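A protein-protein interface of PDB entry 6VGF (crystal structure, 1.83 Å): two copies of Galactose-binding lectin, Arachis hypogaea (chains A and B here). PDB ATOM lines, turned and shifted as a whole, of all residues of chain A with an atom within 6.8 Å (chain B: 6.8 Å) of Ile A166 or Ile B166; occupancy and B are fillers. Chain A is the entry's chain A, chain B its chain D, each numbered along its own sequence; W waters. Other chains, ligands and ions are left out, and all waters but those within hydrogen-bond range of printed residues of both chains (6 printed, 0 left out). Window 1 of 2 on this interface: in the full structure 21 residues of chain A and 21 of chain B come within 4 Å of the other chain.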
ATOM      1  N   SER A  64      -0.035 -15.262 -16.824  1.00  0.00           N
ATOM      2  CA  SER A  64       0.977 -14.757 -17.740  1.00  0.00           C
ATOM      3  C   SER A  64       1.979 -15.876 -17.868  1.00  0.00           C
ATOM      4  O   SER A  64       2.048 -16.720 -16.961  1.00  0.00           O
ATOM      5  CB  SER A  64       1.636 -13.471 -17.217  1.00  0.00           C
ATOM      6  OG  SER A  64       0.800 -12.341 -17.412  1.00  0.00           O
ATOM      7  N   PHE A  65       2.768 -15.894 -18.932  1.00  0.00           N
ATOM      8  CA  PHE A  65       3.828 -16.880 -19.049  1.00  0.00           C
ATOM      9  C   PHE A  65       5.013 -16.355 -19.857  1.00  0.00           C
ATOM     10  O   PHE A  65       4.875 -15.460 -20.703  1.00  0.00           O
ATOM     11  CB  PHE A  65       3.349 -18.242 -19.570  1.00  0.00           C
ATOM     12  CG  PHE A  65       2.817 -18.318 -20.974  1.00  0.00           C
ATOM     13  CD1 PHE A  65       3.688 -18.346 -22.065  1.00  0.00           C
ATOM     14  CD2 PHE A  65       1.458 -18.481 -21.210  1.00  0.00           C
ATOM     15  CE1 PHE A  65       3.207 -18.461 -23.364  1.00  0.00           C
ATOM     16  CE2 PHE A  65       0.971 -18.613 -22.518  1.00  0.00           C
ATOM     17  CZ  PHE A  65       1.839 -18.587 -23.583  1.00  0.00           C
ATOM     18  N   LEU A  66       6.181 -16.941 -19.562  1.00  0.00           N
ATOM     19  CA  LEU A  66       7.443 -16.715 -20.247  1.00  0.00           C
ATOM     20  C   LEU A  66       7.973 -18.077 -20.630  1.00  0.00           C
ATOM     21  O   LEU A  66       8.116 -18.950 -19.768  1.00  0.00           O
ATOM     22  CB  LEU A  66       8.457 -15.955 -19.388  1.00  0.00           C
ATOM     23  CG  LEU A  66       9.906 -15.939 -19.924  1.00  0.00           C
ATOM     24  CD1 LEU A  66      10.035 -15.039 -21.206  1.00  0.00           C
ATOM     25  CD2 LEU A  66      10.864 -15.486 -18.877  1.00  0.00           C
ATOM     26  N   THR A  67       8.262 -18.270 -21.905  1.00  0.00           N
ATOM     27  CA  THR A  67       8.789 -19.578 -22.332  1.00  0.00           C
ATOM     28  C   THR A  67       9.841 -19.379 -23.399  1.00  0.00           C
ATOM     29  O   THR A  67       9.740 -18.486 -24.240  1.00  0.00           O
ATOM     30  CB  THR A  67       7.669 -20.568 -22.757  1.00  0.00           C
ATOM     31  OG1 THR A  67       8.263 -21.834 -23.059  1.00  0.00           O
ATOM     32  CG2 THR A  67       6.829 -20.093 -23.959  1.00  0.00           C
ATOM     33  N   THR A 164      11.735 -16.939 -27.902  1.00  0.00           N
ATOM     34  CA  THR A 164      11.283 -16.450 -26.621  1.00  0.00           C
ATOM     35  C   THR A 164       9.852 -15.975 -26.824  1.00  0.00           C
ATOM     36  O   THR A 164       9.553 -15.267 -27.783  1.00  0.00           O
ATOM     37  CB  THR A 164      12.222 -15.372 -26.041  1.00  0.00           C
ATOM     38  OG1 THR A 164      13.428 -16.011 -25.627  1.00  0.00           O
ATOM     39  CG2 THR A 164      11.613 -14.695 -24.827  1.00  0.00           C
ATOM     40  N   VAL A 165       8.966 -16.413 -25.939  1.00  0.00           N
ATOM     41  CA  VAL A 165       7.564 -16.042 -26.005  1.00  0.00           C
ATOM     42  C   VAL A 165       7.120 -15.468 -24.658  1.00  0.00           C
ATOM     43  O   VAL A 165       7.367 -16.043 -23.597  1.00  0.00           O
ATOM     44  CB  VAL A 165       6.648 -17.217 -26.453  1.00  0.00           C
ATOM     45  CG1 VAL A 165       5.201 -16.767 -26.552  1.00  0.00           C
ATOM     46  CG2 VAL A 165       7.120 -17.852 -27.778  1.00  0.00           C
ATOM     47  N   ILE A 166       6.425 -14.328 -24.722  1.00  0.00           N
ATOM     48  CA  ILE A 166       5.844 -13.679 -23.542  1.00  0.00           C
ATOM     49  C   ILE A 166       4.352 -13.586 -23.763  1.00  0.00           C
ATOM     50  O   ILE A 166       3.912 -13.017 -24.770  1.00  0.00           O
ATOM     51  CB  ILE A 166       6.434 -12.265 -23.228  1.00  0.00           C
ATOM     52  CG1 ILE A 166       7.968 -12.296 -22.955  1.00  0.00           C
ATOM     53  CG2 ILE A 166       5.684 -11.597 -22.047  1.00  0.00           C
ATOM     54  CD1 ILE A 166       8.633 -10.861 -23.018  1.00  0.00           C
ATOM     55  N   TYR A 167       3.571 -14.084 -22.794  1.00  0.00           N
ATOM     56  CA  TYR A 167       2.149 -13.848 -22.817  1.00  0.00           C
ATOM     57  C   TYR A 167       1.815 -12.966 -21.632  1.00  0.00           C
ATOM     58  O   TYR A 167       2.041 -13.347 -20.480  1.00  0.00           O
ATOM     59  CB  TYR A 167       1.310 -15.126 -22.841  1.00  0.00           C
ATOM     60  CG  TYR A 167      -0.172 -14.826 -22.936  1.00  0.00           C
ATOM     61  CD1 TYR A 167      -0.736 -14.358 -24.128  1.00  0.00           C
ATOM     62  CD2 TYR A 167      -0.991 -14.889 -21.806  1.00  0.00           C
ATOM     63  CE1 TYR A 167      -2.084 -14.014 -24.205  1.00  0.00           C
ATOM     64  CE2 TYR A 167      -2.346 -14.564 -21.878  1.00  0.00           C
ATOM     65  CZ  TYR A 167      -2.894 -14.152 -23.085  1.00  0.00           C
ATOM     66  OH  TYR A 167      -4.230 -13.848 -23.172  1.00  0.00           O
ATOM     67  N   ASP A 168       1.338 -11.767 -21.917  1.00  0.00           N
ATOM     68  CA  ASP A 168       0.939 -10.819 -20.878  1.00  0.00           C
ATOM     69  C   ASP A 168      -0.587 -10.893 -20.713  1.00  0.00           C
ATOM     70  O   ASP A 168      -1.324 -10.439 -21.590  1.00  0.00           O
ATOM     71  CB  ASP A 168       1.403  -9.399 -21.240  1.00  0.00           C
ATOM     72  CG  ASP A 168       0.909  -8.374 -20.240  1.00  0.00           C
ATOM     73  OD1 ASP A 168       1.355  -8.411 -19.086  1.00  0.00           O
ATOM     74  OD2 ASP A 168       0.015  -7.596 -20.589  1.00  0.00           O
ATOM     75  N   THR A 173      -1.673 -10.017 -24.767  1.00  0.00           N
ATOM     76  CA  THR A 173      -0.690  -9.978 -25.849  1.00  0.00           C
ATOM     77  C   THR A 173       0.244 -11.167 -25.804  1.00  0.00           C
ATOM     78  O   THR A 173       0.888 -11.408 -24.790  1.00  0.00           O
ATOM     79  CB  THR A 173       0.143  -8.653 -25.812  1.00  0.00           C
ATOM     80  OG1 THR A 173      -0.753  -7.539 -25.936  1.00  0.00           O
ATOM     81  CG2 THR A 173       1.159  -8.589 -26.942  1.00  0.00           C
ATOM     82  N   LEU A 174       0.297 -11.901 -26.924  1.00  0.00           N
ATOM     83  CA  LEU A 174       1.244 -12.980 -27.174  1.00  0.00           C
ATOM     84  C   LEU A 174       2.388 -12.369 -28.037  1.00  0.00           C
ATOM     85  O   LEU A 174       2.147 -12.006 -29.198  1.00  0.00           O
ATOM     86  CB  LEU A 174       0.555 -14.169 -27.894  1.00  0.00           C
ATOM     87  CG  LEU A 174       1.392 -15.422 -28.080  1.00  0.00           C
ATOM     88  CD1 LEU A 174       1.659 -16.115 -26.758  1.00  0.00           C
ATOM     89  CD2 LEU A 174       0.699 -16.417 -29.038  1.00  0.00           C
ATOM     90  N   SER A 175       3.574 -12.181 -27.443  1.00  0.00           N
ATOM     91  CA  SER A 175       4.734 -11.620 -28.129  1.00  0.00           C
ATOM     92  C   SER A 175       5.795 -12.698 -28.350  1.00  0.00           C
ATOM     93  O   SER A 175       6.095 -13.460 -27.440  1.00  0.00           O
ATOM     94  CB  SER A 175       5.306 -10.442 -27.350  1.00  0.00           C
ATOM     95  OG  SER A 175       6.201  -9.783 -28.217  1.00  0.00           O
ATOM     96  N   VAL A 176       6.336 -12.766 -29.579  1.00  0.00           N
ATOM     97  CA  VAL A 176       7.291 -13.804 -30.022  1.00  0.00           C
ATOM     98  C   VAL A 176       8.548 -13.155 -30.614  1.00  0.00           C
ATOM     99  O   VAL A 176       8.438 -12.313 -31.513  1.00  0.00           O
ATOM    100  CB  VAL A 176       6.623 -14.751 -31.081  1.00  0.00           C
ATOM    101  CG1 VAL A 176       7.580 -15.859 -31.541  1.00  0.00           C
ATOM    102  CG2 VAL A 176       5.318 -15.347 -30.570  1.00  0.00           C
ATOM    103  N   ALA A 177       9.734 -13.586 -30.139  1.00  0.00           N
ATOM    104  CA  ALA A 177      11.018 -13.142 -30.687  1.00  0.00           C
ATOM    105  C   ALA A 177      11.795 -14.393 -31.108  1.00  0.00           C
ATOM    106  O   ALA A 177      11.991 -15.299 -30.290  1.00  0.00           O
ATOM    107  CB  ALA A 177      11.801 -12.302 -29.677  1.00  0.00           C
ATOM    108  N   THR A 187      10.274 -10.698 -35.086  1.00  0.00           N
ATOM    109  CA  THR A 187       9.253 -10.632 -34.041  1.00  0.00           C
ATOM    110  C   THR A 187       7.868 -10.642 -34.630  1.00  0.00           C
ATOM    111  O   THR A 187       7.654 -10.207 -35.772  1.00  0.00           O
ATOM    112  CB  THR A 187       9.402  -9.407 -33.098  1.00  0.00           C
ATOM    113  OG1 THR A 187       9.116  -8.198 -33.812  1.00  0.00           O
ATOM    114  CG2 THR A 187      10.753  -9.341 -32.378  1.00  0.00           C
ATOM    115  N   ILE A 188       6.908 -11.104 -33.821  1.00  0.00           N
ATOM    116  CA  ILE A 188       5.483 -11.095 -34.174  1.00  0.00           C
ATOM    117  C   ILE A 188       4.704 -11.075 -32.859  1.00  0.00           C
ATOM    118  O   ILE A 188       5.043 -11.801 -31.929  1.00  0.00           O
ATOM    119  CB  ILE A 188       5.044 -12.239 -35.136  1.00  0.00           C
ATOM    120  CG1 ILE A 188       3.584 -12.018 -35.633  1.00  0.00           C
ATOM    121  CG2 ILE A 188       5.280 -13.657 -34.539  1.00  0.00           C
ATOM    122  CD1 ILE A 188       3.130 -12.957 -36.766  1.00  0.00           C
ATOM    123  N   ALA A 189       3.673 -10.248 -32.791  1.00  0.00           N
ATOM    124  CA  ALA A 189       2.834 -10.119 -31.602  1.00  0.00           C
ATOM    125  C   ALA A 189       1.363 -10.029 -32.024  1.00  0.00           C
ATOM    126  O   ALA A 189       1.053  -9.528 -33.097  1.00  0.00           O
ATOM    127  CB  ALA A 189       3.266  -8.911 -30.746  1.00  0.00           C
ATOM    128  N   SER B  64      12.752  -3.989 -34.434  1.00  0.00           N
ATOM    129  CA  SER B  64      12.263  -4.816 -33.357  1.00  0.00           C
ATOM    130  C   SER B  64      13.488  -5.097 -32.494  1.00  0.00           C
ATOM    131  O   SER B  64      14.609  -5.027 -33.002  1.00  0.00           O
ATOM    132  CB  SER B  64      11.637  -6.113 -33.888  1.00  0.00           C
ATOM    133  OG  SER B  64      10.320  -5.903 -34.389  1.00  0.00           O
ATOM    134  N   PHE B  65      13.299  -5.420 -31.212  1.00  0.00           N
ATOM    135  CA  PHE B  65      14.444  -5.812 -30.397  1.00  0.00           C
ATOM    136  C   PHE B  65      14.067  -6.813 -29.326  1.00  0.00           C
ATOM    137  O   PHE B  65      12.910  -6.898 -28.899  1.00  0.00           O
ATOM    138  CB  PHE B  65      15.206  -4.607 -29.787  1.00  0.00           C
ATOM    139  CG  PHE B  65      14.486  -3.750 -28.782  1.00  0.00           C
ATOM    140  CD1 PHE B  65      14.341  -4.170 -27.463  1.00  0.00           C
ATOM    141  CD2 PHE B  65      14.042  -2.475 -29.122  1.00  0.00           C
ATOM    142  CE1 PHE B  65      13.717  -3.356 -26.519  1.00  0.00           C
ATOM    143  CE2 PHE B  65      13.442  -1.653 -28.169  1.00  0.00           C
ATOM    144  CZ  PHE B  65      13.258  -2.109 -26.884  1.00  0.00           C
ATOM    145  N   LEU B  66      15.076  -7.575 -28.903  1.00  0.00           N
ATOM    146  CA  LEU B  66      15.004  -8.546 -27.826  1.00  0.00           C
ATOM    147  C   LEU B  66      16.159  -8.269 -26.901  1.00  0.00           C
ATOM    148  O   LEU B  66      17.311  -8.240 -27.342  1.00  0.00           O
ATOM    149  CB  LEU B  66      15.048  -9.993 -28.345  1.00  0.00           C
ATOM    150  CG  LEU B  66      15.283 -11.084 -27.274  1.00  0.00           C
ATOM    151  CD1 LEU B  66      14.073 -11.250 -26.346  1.00  0.00           C
ATOM    152  CD2 LEU B  66      15.642 -12.432 -27.950  1.00  0.00           C
ATOM    153  N   THR B  67      15.878  -8.093 -25.618  1.00  0.00           N
ATOM    154  CA  THR B  67      16.961  -7.825 -24.682  1.00  0.00           C
ATOM    155  C   THR B  67      16.694  -8.525 -23.365  1.00  0.00           C
ATOM    156  O   THR B  67      15.551  -8.622 -22.911  1.00  0.00           O
ATOM    157  CB  THR B  67      17.247  -6.304 -24.522  1.00  0.00           C
ATOM    158  OG1 THR B  67      18.374  -6.125 -23.677  1.00  0.00           O
ATOM    159  CG2 THR B  67      16.051  -5.489 -23.977  1.00  0.00           C
ATOM    160  N   THR B 164      13.338 -10.037 -19.327  1.00  0.00           N
ATOM    161  CA  THR B 164      13.332 -10.240 -20.763  1.00  0.00           C
ATOM    162  C   THR B 164      12.353  -9.202 -21.353  1.00  0.00           C
ATOM    163  O   THR B 164      11.229  -9.036 -20.852  1.00  0.00           O
ATOM    164  CB  THR B 164      12.983 -11.671 -21.149  1.00  0.00           C
ATOM    165  OG1 THR B 164      14.078 -12.514 -20.796  1.00  0.00           O
ATOM    166  CG2 THR B 164      12.707 -11.792 -22.630  1.00  0.00           C
ATOM    167  N   VAL B 165      12.817  -8.479 -22.377  1.00  0.00           N
ATOM    168  CA  VAL B 165      12.017  -7.445 -23.016  1.00  0.00           C
ATOM    169  C   VAL B 165      11.964  -7.694 -24.517  1.00  0.00           C
ATOM    170  O   VAL B 165      13.000  -7.890 -25.148  1.00  0.00           O
ATOM    171  CB  VAL B 165      12.519  -5.996 -22.698  1.00  0.00           C
ATOM    172  CG1 VAL B 165      11.596  -4.952 -23.339  1.00  0.00           C
ATOM    173  CG2 VAL B 165      12.643  -5.748 -21.191  1.00  0.00           C
ATOM    174  N   ILE B 166      10.753  -7.625 -25.086  1.00  0.00           N
ATOM    175  CA  ILE B 166      10.524  -7.747 -26.516  1.00  0.00           C
ATOM    176  C   ILE B 166       9.851  -6.471 -26.994  1.00  0.00           C
ATOM    177  O   ILE B 166       8.792  -6.091 -26.480  1.00  0.00           O
ATOM    178  CB  ILE B 166       9.678  -8.995 -26.939  1.00  0.00           C
ATOM    179  CG1 ILE B 166      10.293 -10.337 -26.465  1.00  0.00           C
ATOM    180  CG2 ILE B 166       9.408  -9.005 -28.466  1.00  0.00           C
ATOM    181  CD1 ILE B 166       9.342 -11.573 -26.599  1.00  0.00           C
ATOM    182  N   TYR B 167      10.401  -5.887 -28.046  1.00  0.00           N
ATOM    183  CA  TYR B 167       9.713  -4.802 -28.720  1.00  0.00           C
ATOM    184  C   TYR B 167       9.366  -5.273 -30.127  1.00  0.00           C
ATOM    185  O   TYR B 167      10.252  -5.556 -30.932  1.00  0.00           O
ATOM    186  CB  TYR B 167      10.482  -3.488 -28.718  1.00  0.00           C
ATOM    187  CG  TYR B 167       9.693  -2.382 -29.360  1.00  0.00           C
ATOM    188  CD1 TYR B 167       8.605  -1.806 -28.704  1.00  0.00           C
ATOM    189  CD2 TYR B 167       9.940  -1.993 -30.678  1.00  0.00           C
ATOM    190  CE1 TYR B 167       7.829  -0.818 -29.320  1.00  0.00           C
ATOM    191  CE2 TYR B 167       9.186  -0.981 -31.292  1.00  0.00           C
ATOM    192  CZ  TYR B 167       8.138  -0.395 -30.600  1.00  0.00           C
ATOM    193  OH  TYR B 167       7.386   0.602 -31.177  1.00  0.00           O
ATOM    194  N   ASP B 168       8.070  -5.374 -30.405  1.00  0.00           N
ATOM    195  CA  ASP B 168       7.580  -5.777 -31.708  1.00  0.00           C
ATOM    196  C   ASP B 168       7.190  -4.508 -32.499  1.00  0.00           C
ATOM    197  O   ASP B 168       6.175  -3.879 -32.178  1.00  0.00           O
ATOM    198  CB  ASP B 168       6.399  -6.730 -31.562  1.00  0.00           C
ATOM    199  CG  ASP B 168       5.806  -7.070 -32.906  1.00  0.00           C
ATOM    200  OD1 ASP B 168       6.493  -7.739 -33.699  1.00  0.00           O
ATOM    201  OD2 ASP B 168       4.693  -6.609 -33.189  1.00  0.00           O
ATOM    202  N   THR B 173       4.411  -2.856 -29.733  1.00  0.00           N
ATOM    203  CA  THR B 173       4.234  -3.402 -28.388  1.00  0.00           C
ATOM    204  C   THR B 173       5.539  -3.655 -27.703  1.00  0.00           C
ATOM    205  O   THR B 173       6.370  -4.408 -28.212  1.00  0.00           O
ATOM    206  CB  THR B 173       3.395  -4.705 -28.421  1.00  0.00           C
ATOM    207  OG1 THR B 173       2.129  -4.393 -29.024  1.00  0.00           O
ATOM    208  CG2 THR B 173       3.195  -5.303 -27.032  1.00  0.00           C
ATOM    209  N   LEU B 174       5.675  -3.058 -26.514  1.00  0.00           N
ATOM    210  CA  LEU B 174       6.777  -3.278 -25.574  1.00  0.00           C
ATOM    211  C   LEU B 174       6.277  -4.296 -24.521  1.00  0.00           C
ATOM    212  O   LEU B 174       5.326  -4.008 -23.777  1.00  0.00           O
ATOM    213  CB  LEU B 174       7.230  -1.952 -24.924  1.00  0.00           C
ATOM    214  CG  LEU B 174       8.547  -1.997 -24.114  1.00  0.00           C
ATOM    215  CD1 LEU B 174       9.768  -2.226 -25.004  1.00  0.00           C
ATOM    216  CD2 LEU B 174       8.723  -0.749 -23.287  1.00  0.00           C
ATOM    217  N   SER B 175       6.827  -5.523 -24.540  1.00  0.00           N
ATOM    218  CA  SER B 175       6.440  -6.581 -23.590  1.00  0.00           C
ATOM    219  C   SER B 175       7.606  -6.881 -22.656  1.00  0.00           C
ATOM    220  O   SER B 175       8.759  -7.018 -23.114  1.00  0.00           O
ATOM    221  CB  SER B 175       6.020  -7.836 -24.341  1.00  0.00           C
ATOM    222  OG  SER B 175       4.874  -7.610 -25.142  1.00  0.00           O
ATOM    223  N   VAL B 176       7.315  -6.997 -21.349  1.00  0.00           N
ATOM    224  CA  VAL B 176       8.310  -7.200 -20.284  1.00  0.00           C
ATOM    225  C   VAL B 176       7.926  -8.408 -19.414  1.00  0.00           C
ATOM    226  O   VAL B 176       6.790  -8.493 -18.935  1.00  0.00           O
ATOM    227  CB  VAL B 176       8.428  -5.910 -19.399  1.00  0.00           C
ATOM    228  CG1 VAL B 176       9.476  -6.057 -18.295  1.00  0.00           C
ATOM    229  CG2 VAL B 176       8.708  -4.655 -20.242  1.00  0.00           C
ATOM    230  N   ALA B 177       8.879  -9.322 -19.191  1.00  0.00           N
ATOM    231  CA  ALA B 177       8.711 -10.470 -18.281  1.00  0.00           C
ATOM    232  C   ALA B 177       9.843 -10.417 -17.251  1.00  0.00           C
ATOM    233  O   ALA B 177      11.030 -10.340 -17.613  1.00  0.00           O
ATOM    234  CB  ALA B 177       8.696 -11.790 -19.041  1.00  0.00           C
ATOM    235  N   THR B 187       4.514  -9.811 -15.530  1.00  0.00           N
ATOM    236  CA  THR B 187       4.563  -9.279 -16.895  1.00  0.00           C
ATOM    237  C   THR B 187       3.840  -7.955 -16.959  1.00  0.00           C
ATOM    238  O   THR B 187       2.924  -7.693 -16.161  1.00  0.00           O
ATOM    239  CB  THR B 187       3.992 -10.233 -17.958  1.00  0.00           C
ATOM    240  OG1 THR B 187       2.576 -10.362 -17.788  1.00  0.00           O
ATOM    241  CG2 THR B 187       4.701 -11.578 -18.024  1.00  0.00           C
ATOM    242  N   ILE B 188       4.231  -7.147 -17.948  1.00  0.00           N
ATOM    243  CA  ILE B 188       3.589  -5.869 -18.267  1.00  0.00           C
ATOM    244  C   ILE B 188       3.887  -5.589 -19.733  1.00  0.00           C
ATOM    245  O   ILE B 188       5.036  -5.743 -20.179  1.00  0.00           O
ATOM    246  CB  ILE B 188       4.008  -4.696 -17.317  1.00  0.00           C
ATOM    247  CG1 ILE B 188       3.143  -3.426 -17.598  1.00  0.00           C
ATOM    248  CG2 ILE B 188       5.544  -4.412 -17.319  1.00  0.00           C
ATOM    249  CD1 ILE B 188       3.310  -2.289 -16.572  1.00  0.00           C
ATOM    250  N   ALA B 189       2.852  -5.176 -20.471  1.00  0.00           N
ATOM    251  CA  ALA B 189       2.988  -4.816 -21.883  1.00  0.00           C
ATOM    252  C   ALA B 189       2.212  -3.535 -22.174  1.00  0.00           C
ATOM    253  O   ALA B 189       1.184  -3.266 -21.538  1.00  0.00           O
ATOM    254  CB  ALA B 189       2.520  -5.952 -22.777  1.00  0.00           C
HETATM  255  O   HOH W   1      -0.417  -9.205 -17.115  1.00  0.00           O
HETATM  256  O   HOH W   2       3.434  -9.874 -24.373  1.00  0.00           O
HETATM  257  O   HOH W   3       7.310  -6.439 -36.097  1.00  0.00           O
HETATM  258  O   HOH W   4       0.254  -5.340 -18.900  1.00  0.00           O
HETATM  259  O   HOH W   5       3.280  -8.348 -35.085  1.00  0.00           O
HETATM  260  O   HOH W   6       5.841  -7.223 -27.753  1.00  0.00           O
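Water W6 lies within hydrogen-bond range of OG of Ser A175, OG of Ser B175, O of Thr B173 and O of Ile B166.
Water W1 lies within hydrogen-bond range of the side-chain carboxylate (OD1) of Asp A168, the side-chain hydroxyl (OG1) of Thr B187 and the side-chain hydroxyl (OG) of Ser A64.
Water W2 lies within hydrogen-bond range of the side-chain hydroxyl (OG) of Ser B175, the backbone carbonyl oxygen (O) of Thr A173 and the backbone carbonyl oxygen (O) of Ile A166.
Water W4 lies within hydrogen-bond range of the side-chain carboxylate of Asp A168 and the backbone NH of Ala B189.
Water W3 bridges the side-chain carboxylate (OD1) of Asp B168 (2.8 Å) and the side-chain hydroxyl (OG1) of Thr A187 (3.4 Å).
Water W5 lies within hydrogen-bond range of OD2 of Asp B168 (2.9 Å) and N of Ala A189 (3.0 Å).
Of the printed residues of chain B, Ile A166 touches Thr B164, Ile B166 and Ser B175.
Printed residues of chain A within 4 Å of Ile B166: Thr A164 (3.9 Å), Ile A166 (3.7 Å) and Ser A175 (3.3 Å).
Printed residues of chain B within 4 Å of Thr A187: Ser B64 and Asp B168.
Of the printed residues of chain A, Thr B164 touches Thr A164 (3.8 Å) and Ile A166 (3.8 Å).
Of the printed residues of chain A, Ala B189 touches Asp A168.
Leu A66 touches none of the printed residues of chain B.
Thr B67 touches none of the printed residues of chain A.
The nearest printed residue of chain A that does not touch Ile B166 is Ala A177 (4.01 Å).
Of the 17 printed residues of chain B, 9 touch a printed residue of chain A.
Among the printed residues, 16 pairs touch across the chains.
Thr A164 touches Ile B166, and with the chains exchanged Ile A166 touches Thr B164.
Asp A168 touches Thr B187, and with the chains exchanged Thr A187 touches Asp B168.
Asp A168 touches Ile B188, and with the chains exchanged Ile A188 touches Asp B168.
Asp A168 touches Ala B189, and with the chains exchanged Ala A189 touches Asp B168.
17 positions are printed for both chains.
Of the 16 pairs that touch across the chains among the printed residues, 16 have their exchanged pair printed and touching as well.
Among the printed residues, merely in contact across the chains: Thr A164 with Thr B164, Thr A164 with Ile B166, Ile A166 with Thr B164, Ile A166 with Ile B166, Ile A166 with Ser B175, Asp A168 with Ala B189, Thr A173 with Thr B173, Ser A175 with Ile B166, Ser A175 with Ser B175 and Ala A189 with Asp B168.
O of Tyr A167 sits close to OG of Ser A64 (3.5 Å).
O of Ile B166 sits at hydrogen-bond distance from N of Ser B175, 2.8 Å away.
The backbone NH (N) of Asp A168 sits at hydrogen-bond distance from the backbone carbonyl oxygen (O) of Thr A173, 2.9 Å away.
The backbone NH (N) of Thr B164 sits at hydrogen-bond distance from the backbone carbonyl oxygen (O) of Ala B177, 2.9 Å away.
O of Tyr B167 sits close to OG of Ser B64, at 3.5 Å.
O of Thr A164 sits at hydrogen-bond distance from N of Ala A177 (2.9 Å).
The side-chain carboxylate (OD1) of Asp A168 sits at hydrogen-bond distance from the side-chain hydroxyl (OG1) of Thr B187 (2.6 Å).
OG1 of Thr A187 lies within hydrogen-bond range of OG of Ser B64 (2.7 Å).
The side-chain carboxylate of Asp B168 lies within hydrogen-bond range of the side-chain hydroxyl of Thr A187, 2.7 Å away.
The side-chain carboxylate of Asp A168 sits at hydrogen-bond distance from the backbone NH of Ile B188, 3.3 Å away.
OD1 of Asp B168 sits at hydrogen-bond distance from N of Ile A188.
The side-chain hydroxyl (OG) of Ser A64 is in hydrogen-bond range of the side-chain hydroxyl (OG1) of Thr B187, 2.7 Å away.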
